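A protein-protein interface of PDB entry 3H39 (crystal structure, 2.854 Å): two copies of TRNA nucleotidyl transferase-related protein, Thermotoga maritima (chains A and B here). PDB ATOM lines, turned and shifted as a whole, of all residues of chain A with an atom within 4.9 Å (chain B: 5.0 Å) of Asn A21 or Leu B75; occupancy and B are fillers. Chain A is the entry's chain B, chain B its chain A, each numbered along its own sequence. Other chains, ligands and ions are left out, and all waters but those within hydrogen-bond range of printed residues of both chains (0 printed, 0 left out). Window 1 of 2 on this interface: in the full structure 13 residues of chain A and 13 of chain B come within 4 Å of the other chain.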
ATOM      1  N   PRO A  17      29.427  -1.166  -1.972  1.00  0.00           N
ATOM      2  CA  PRO A  17      29.570  -1.794  -3.296  1.00  0.00           C
ATOM      3  C   PRO A  17      30.696  -2.831  -3.420  1.00  0.00           C
ATOM      4  O   PRO A  17      30.444  -3.911  -3.942  1.00  0.00           O
ATOM      5  CB  PRO A  17      29.790  -0.598  -4.223  1.00  0.00           C
ATOM      6  CG  PRO A  17      28.986   0.468  -3.576  1.00  0.00           C
ATOM      7  CD  PRO A  17      29.210   0.286  -2.091  1.00  0.00           C
ATOM      8  N   LYS A  18      31.900  -2.527  -2.951  1.00  0.00           N
ATOM      9  CA  LYS A  18      32.954  -3.537  -2.917  1.00  0.00           C
ATOM     10  C   LYS A  18      32.433  -4.837  -2.298  1.00  0.00           C
ATOM     11  O   LYS A  18      32.670  -5.915  -2.829  1.00  0.00           O
ATOM     12  CB  LYS A  18      34.203  -3.041  -2.163  1.00  0.00           C
ATOM     13  CG  LYS A  18      35.044  -1.993  -2.907  1.00  0.00           C
ATOM     14  CD  LYS A  18      34.847  -0.570  -2.360  1.00  0.00           C
ATOM     15  CE  LYS A  18      35.615  -0.365  -1.047  1.00  0.00           C
ATOM     16  NZ  LYS A  18      35.712   1.069  -0.639  1.00  0.00           N
ATOM     17  N   ILE A  19      31.750  -4.745  -1.177  1.00  0.00           N
ATOM     18  CA  ILE A  19      31.182  -5.923  -0.548  1.00  0.00           C
ATOM     19  C   ILE A  19      30.032  -6.582  -1.273  1.00  0.00           C
ATOM     20  O   ILE A  19      30.035  -7.774  -1.475  1.00  0.00           O
ATOM     21  CB  ILE A  19      30.821  -5.605   0.860  1.00  0.00           C
ATOM     22  CG1 ILE A  19      32.050  -5.008   1.509  1.00  0.00           C
ATOM     23  CG2 ILE A  19      30.436  -6.834   1.581  1.00  0.00           C
ATOM     24  CD1 ILE A  19      31.878  -4.737   2.900  1.00  0.00           C
ATOM     25  N   LEU A  20      29.066  -5.801  -1.715  1.00  0.00           N
ATOM     26  CA  LEU A  20      28.017  -6.344  -2.573  1.00  0.00           C
ATOM     27  C   LEU A  20      28.611  -7.173  -3.692  1.00  0.00           C
ATOM     28  O   LEU A  20      28.229  -8.324  -3.893  1.00  0.00           O
ATOM     29  CB  LEU A  20      27.185  -5.236  -3.196  1.00  0.00           C
ATOM     30  CG  LEU A  20      25.752  -5.063  -2.697  1.00  0.00           C
ATOM     31  CD1 LEU A  20      24.946  -4.337  -3.755  1.00  0.00           C
ATOM     32  CD2 LEU A  20      25.084  -6.397  -2.328  1.00  0.00           C
ATOM     33  N   ASN A  21      29.553  -6.585  -4.423  1.00  0.00           N
ATOM     34  CA  ASN A  21      30.177  -7.279  -5.552  1.00  0.00           C
ATOM     35  C   ASN A  21      30.841  -8.570  -5.125  1.00  0.00           C
ATOM     36  O   ASN A  21      30.916  -9.529  -5.892  1.00  0.00           O
ATOM     37  CB  ASN A  21      31.176  -6.384  -6.287  1.00  0.00           C
ATOM     38  CG  ASN A  21      30.502  -5.346  -7.130  1.00  0.00           C
ATOM     39  OD1 ASN A  21      29.311  -5.439  -7.419  1.00  0.00           O
ATOM     40  ND2 ASN A  21      31.251  -4.346  -7.529  1.00  0.00           N
ATOM     41  N   LEU A  22      31.321  -8.582  -3.889  1.00  0.00           N
ATOM     42  CA  LEU A  22      31.850  -9.793  -3.283  1.00  0.00           C
ATOM     43  C   LEU A  22      30.732 -10.814  -3.144  1.00  0.00           C
ATOM     44  O   LEU A  22      30.864 -11.968  -3.567  1.00  0.00           O
ATOM     45  CB  LEU A  22      32.412  -9.462  -1.908  1.00  0.00           C
ATOM     46  CG  LEU A  22      33.819  -9.955  -1.645  1.00  0.00           C
ATOM     47  CD1 LEU A  22      34.425 -10.472  -2.933  1.00  0.00           C
ATOM     48  CD2 LEU A  22      34.604  -8.780  -1.101  1.00  0.00           C
ATOM     49  N   PHE A  23      29.626 -10.369  -2.550  1.00  0.00           N
ATOM     50  CA  PHE A  23      28.489 -11.235  -2.320  1.00  0.00           C
ATOM     51  C   PHE A  23      27.993 -11.853  -3.613  1.00  0.00           C
ATOM     52  O   PHE A  23      27.765 -13.064  -3.660  1.00  0.00           O
ATOM     53  CB  PHE A  23      27.353 -10.493  -1.609  1.00  0.00           C
ATOM     54  CG  PHE A  23      27.569 -10.324  -0.131  1.00  0.00           C
ATOM     55  CD1 PHE A  23      28.310 -11.243   0.583  1.00  0.00           C
ATOM     56  CD2 PHE A  23      27.014  -9.258   0.545  1.00  0.00           C
ATOM     57  CE1 PHE A  23      28.505 -11.089   1.943  1.00  0.00           C
ATOM     58  CE2 PHE A  23      27.211  -9.109   1.901  1.00  0.00           C
ATOM     59  CZ  PHE A  23      27.956 -10.025   2.599  1.00  0.00           C
ATOM     60  N   ARG A  24      27.828 -11.028  -4.648  1.00  0.00           N
ATOM     61  CA  ARG A  24      27.434 -11.513  -5.975  1.00  0.00           C
ATOM     62  C   ARG A  24      28.448 -12.501  -6.541  1.00  0.00           C
ATOM     63  O   ARG A  24      28.083 -13.531  -7.114  1.00  0.00           O
ATOM     64  CB  ARG A  24      27.303 -10.363  -6.963  1.00  0.00           C
ATOM     65  CG  ARG A  24      26.429  -9.236  -6.508  1.00  0.00           C
ATOM     66  CD  ARG A  24      26.590  -8.088  -7.466  1.00  0.00           C
ATOM     67  NE  ARG A  24      25.400  -7.255  -7.517  1.00  0.00           N
ATOM     68  CZ  ARG A  24      25.399  -5.948  -7.313  1.00  0.00           C
ATOM     69  NH1 ARG A  24      26.539  -5.316  -7.062  1.00  0.00           N
ATOM     70  NH2 ARG A  24      24.258  -5.277  -7.381  1.00  0.00           N
ATOM     71  N   LEU A  25      29.728 -12.185  -6.398  1.00  0.00           N
ATOM     72  CA  LEU A  25      30.746 -13.081  -6.918  1.00  0.00           C
ATOM     73  C   LEU A  25      30.699 -14.413  -6.194  1.00  0.00           C
ATOM     74  O   LEU A  25      30.686 -15.475  -6.830  1.00  0.00           O
ATOM     75  CB  LEU A  25      32.133 -12.448  -6.845  1.00  0.00           C
ATOM     76  CG  LEU A  25      32.320 -11.381  -7.921  1.00  0.00           C
ATOM     77  CD1 LEU A  25      33.614 -10.634  -7.744  1.00  0.00           C
ATOM     78  CD2 LEU A  25      32.258 -12.016  -9.281  1.00  0.00           C
ATOM     79  N   LEU B  22      34.347  -9.318 -14.035  1.00  0.00           N
ATOM     80  CA  LEU B  22      33.518  -8.287 -14.632  1.00  0.00           C
ATOM     81  C   LEU B  22      32.378  -8.880 -15.451  1.00  0.00           C
ATOM     82  O   LEU B  22      31.309  -8.278 -15.538  1.00  0.00           O
ATOM     83  CB  LEU B  22      34.379  -7.423 -15.531  1.00  0.00           C
ATOM     84  CG  LEU B  22      33.846  -6.057 -15.908  1.00  0.00           C
ATOM     85  CD1 LEU B  22      33.427  -5.261 -14.670  1.00  0.00           C
ATOM     86  CD2 LEU B  22      34.928  -5.333 -16.690  1.00  0.00           C
ATOM     87  N   LEU B  25      29.675 -10.166 -13.079  1.00  0.00           N
ATOM     88  CA  LEU B  25      28.910  -9.085 -12.481  1.00  0.00           C
ATOM     89  C   LEU B  25      27.935  -8.489 -13.479  1.00  0.00           C
ATOM     90  O   LEU B  25      26.750  -8.353 -13.177  1.00  0.00           O
ATOM     91  CB  LEU B  25      29.820  -7.997 -11.903  1.00  0.00           C
ATOM     92  CG  LEU B  25      30.653  -8.436 -10.703  1.00  0.00           C
ATOM     93  CD1 LEU B  25      31.666  -7.373 -10.305  1.00  0.00           C
ATOM     94  CD2 LEU B  25      29.722  -8.726  -9.577  1.00  0.00           C
ATOM     95  N   LEU B  26      28.429  -8.133 -14.662  1.00  0.00           N
ATOM     96  CA  LEU B  26      27.567  -7.593 -15.701  1.00  0.00           C
ATOM     97  C   LEU B  26      26.357  -8.503 -15.867  1.00  0.00           C
ATOM     98  O   LEU B  26      25.216  -8.047 -15.933  1.00  0.00           O
ATOM     99  CB  LEU B  26      28.325  -7.489 -17.019  1.00  0.00           C
ATOM    100  CG  LEU B  26      29.480  -6.497 -17.079  1.00  0.00           C
ATOM    101  CD1 LEU B  26      30.032  -6.456 -18.491  1.00  0.00           C
ATOM    102  CD2 LEU B  26      29.010  -5.116 -16.639  1.00  0.00           C
ATOM    103  N   PHE B  29      24.122  -7.958 -12.851  1.00  0.00           N
ATOM    104  CA  PHE B  29      23.450  -6.670 -12.978  1.00  0.00           C
ATOM    105  C   PHE B  29      22.326  -6.797 -13.991  1.00  0.00           C
ATOM    106  O   PHE B  29      21.235  -6.276 -13.785  1.00  0.00           O
ATOM    107  CB  PHE B  29      24.386  -5.570 -13.477  1.00  0.00           C
ATOM    108  CG  PHE B  29      25.609  -5.357 -12.639  1.00  0.00           C
ATOM    109  CD1 PHE B  29      26.680  -4.652 -13.152  1.00  0.00           C
ATOM    110  CD2 PHE B  29      25.693  -5.846 -11.355  1.00  0.00           C
ATOM    111  CE1 PHE B  29      27.809  -4.450 -12.401  1.00  0.00           C
ATOM    112  CE2 PHE B  29      26.826  -5.638 -10.607  1.00  0.00           C
ATOM    113  CZ  PHE B  29      27.882  -4.947 -11.130  1.00  0.00           C
ATOM    114  N   ALA B  71      25.214  -0.042 -13.691  1.00  0.00           N
ATOM    115  CA  ALA B  71      26.514  -0.664 -13.434  1.00  0.00           C
ATOM    116  C   ALA B  71      27.526   0.277 -12.761  1.00  0.00           C
ATOM    117  O   ALA B  71      28.210  -0.120 -11.825  1.00  0.00           O
ATOM    118  CB  ALA B  71      27.095  -1.291 -14.696  1.00  0.00           C
ATOM    119  N   LYS B  72      27.624   1.516 -13.230  1.00  0.00           N
ATOM    120  CA  LYS B  72      28.547   2.488 -12.643  1.00  0.00           C
ATOM    121  C   LYS B  72      28.429   2.496 -11.119  1.00  0.00           C
ATOM    122  O   LYS B  72      29.418   2.638 -10.398  1.00  0.00           O
ATOM    123  CB  LYS B  72      28.241   3.891 -13.162  1.00  0.00           C
ATOM    124  CG  LYS B  72      29.464   4.689 -13.610  1.00  0.00           C
ATOM    125  CD  LYS B  72      30.734   4.286 -12.878  1.00  0.00           C
ATOM    126  CE  LYS B  72      30.895   4.988 -11.545  1.00  0.00           C
ATOM    127  NZ  LYS B  72      32.226   4.674 -10.933  1.00  0.00           N
ATOM    128  N   ARG B  73      27.201   2.357 -10.636  1.00  0.00           N
ATOM    129  CA  ARG B  73      26.925   2.309  -9.212  1.00  0.00           C
ATOM    130  C   ARG B  73      27.903   1.414  -8.479  1.00  0.00           C
ATOM    131  O   ARG B  73      28.368   1.741  -7.384  1.00  0.00           O
ATOM    132  CB  ARG B  73      25.516   1.780  -8.993  1.00  0.00           C
ATOM    133  CG  ARG B  73      24.451   2.837  -9.106  1.00  0.00           C
ATOM    134  CD  ARG B  73      23.785   2.999  -7.792  1.00  0.00           C
ATOM    135  NE  ARG B  73      22.480   2.353  -7.787  1.00  0.00           N
ATOM    136  CZ  ARG B  73      21.961   1.735  -6.729  1.00  0.00           C
ATOM    137  NH1 ARG B  73      22.653   1.650  -5.593  1.00  0.00           N
ATOM    138  NH2 ARG B  73      20.755   1.189  -6.817  1.00  0.00           N
ATOM    139  N   PHE B  74      28.224   0.288  -9.097  1.00  0.00           N
ATOM    140  CA  PHE B  74      28.987  -0.739  -8.414  1.00  0.00           C
ATOM    141  C   PHE B  74      30.360  -0.987  -8.973  1.00  0.00           C
ATOM    142  O   PHE B  74      31.012  -1.915  -8.543  1.00  0.00           O
ATOM    143  CB  PHE B  74      28.208  -2.045  -8.409  1.00  0.00           C
ATOM    144  CG  PHE B  74      26.808  -1.889  -7.924  1.00  0.00           C
ATOM    145  CD1 PHE B  74      25.744  -1.975  -8.799  1.00  0.00           C
ATOM    146  CD2 PHE B  74      26.560  -1.630  -6.587  1.00  0.00           C
ATOM    147  CE1 PHE B  74      24.460  -1.823  -8.350  1.00  0.00           C
ATOM    148  CE2 PHE B  74      25.284  -1.475  -6.131  1.00  0.00           C
ATOM    149  CZ  PHE B  74      24.230  -1.571  -7.011  1.00  0.00           C
ATOM    150  N   LEU B  75      30.802  -0.161  -9.913  1.00  0.00           N
ATOM    151  CA  LEU B  75      32.086  -0.365 -10.598  1.00  0.00           C
ATOM    152  C   LEU B  75      32.872   0.933 -10.712  1.00  0.00           C
ATOM    153  O   LEU B  75      32.356   1.943 -11.179  1.00  0.00           O
ATOM    154  CB  LEU B  75      31.864  -0.898 -12.017  1.00  0.00           C
ATOM    155  CG  LEU B  75      31.807  -2.381 -12.392  1.00  0.00           C
ATOM    156  CD1 LEU B  75      31.523  -3.260 -11.218  1.00  0.00           C
ATOM    157  CD2 LEU B  75      30.754  -2.594 -13.485  1.00  0.00           C
ATOM    158  N   PRO B  76      34.147   0.903 -10.323  1.00  0.00           N
ATOM    159  CA  PRO B  76      34.987   2.094 -10.419  1.00  0.00           C
ATOM    160  C   PRO B  76      35.304   2.421 -11.872  1.00  0.00           C
ATOM    161  O   PRO B  76      35.681   1.532 -12.622  1.00  0.00           O
ATOM    162  CB  PRO B  76      36.259   1.629  -9.727  1.00  0.00           C
ATOM    163  CG  PRO B  76      36.364   0.213 -10.201  1.00  0.00           C
ATOM    164  CD  PRO B  76      34.951  -0.278  -9.961  1.00  0.00           C
ATOM    165  N   GLY B  77      35.174   3.680 -12.260  1.00  0.00           N
ATOM    166  CA  GLY B  77      35.549   4.084 -13.605  1.00  0.00           C
ATOM    167  C   GLY B  77      34.735   5.272 -14.077  1.00  0.00           C
ATOM    168  O   GLY B  77      33.883   5.772 -13.333  1.00  0.00           O
ATOM    169  N   LEU B  92      37.462   1.528 -17.655  1.00  0.00           N
ATOM    170  CA  LEU B  92      38.111   0.877 -16.530  1.00  0.00           C
ATOM    171  C   LEU B  92      39.628   0.844 -16.713  1.00  0.00           C
ATOM    172  O   LEU B  92      40.151   1.066 -17.815  1.00  0.00           O
ATOM    173  CB  LEU B  92      37.565  -0.537 -16.330  1.00  0.00           C
ATOM    174  CG  LEU B  92      36.050  -0.734 -16.147  1.00  0.00           C
ATOM    175  CD1 LEU B  92      35.767  -2.121 -15.587  1.00  0.00           C
ATOM    176  CD2 LEU B  92      35.384   0.331 -15.271  1.00  0.00           C
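The side-chain amide nitrogen of Asn A21 lies within hydrogen-bond range of the backbone carbonyl oxygen of Phe B74 (2.6 Å).
NZ of Lys B72 sits at hydrogen-bond distance from O of Leu B75, at 2.7 Å. The side-chain amide oxygen of Asn A21 is in hydrogen-bond range of the guanidinium group of Arg A24 (2.8 Å).
Among the printed residues, merely in contact across the chains: Arg A24 with Phe B74 (3.5 Å), Arg A24 with Phe B29 (3.6 Å), Leu A20 with Phe B74 (3.7 Å), Arg A24 with Leu B25 (3.8 Å), Asn A21 with Leu B75 (3.9 Å) and Asn A21 with Leu B25 (3.9 Å).
Of the printed residues of chain B, Leu A20 touches Phe B74. Printed residues of chain A within 4 Å of Leu B25: Asn A21 (3.9 Å) and Arg A24 (3.8 Å). Of the printed residues of chain A, Phe B29 touches Arg A24 (3.6 Å). Of the printed residues of chain A, Phe B74 touches Leu A20 (3.7 Å), Asn A21 (2.6 Å) and Arg A24 (3.5 Å). Leu B75 touches just one residue of chain A: Asn A21 (3.9 Å). The nearest printed residue of chain A that does not touch Leu B75 is Pro A17 (5.8 Å).
Among the printed residues, no Asp or Glu carboxylate lies within 4 Å of a Lys or Arg side-chain nitrogen of the other chain.
2 positions are printed for both chains.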
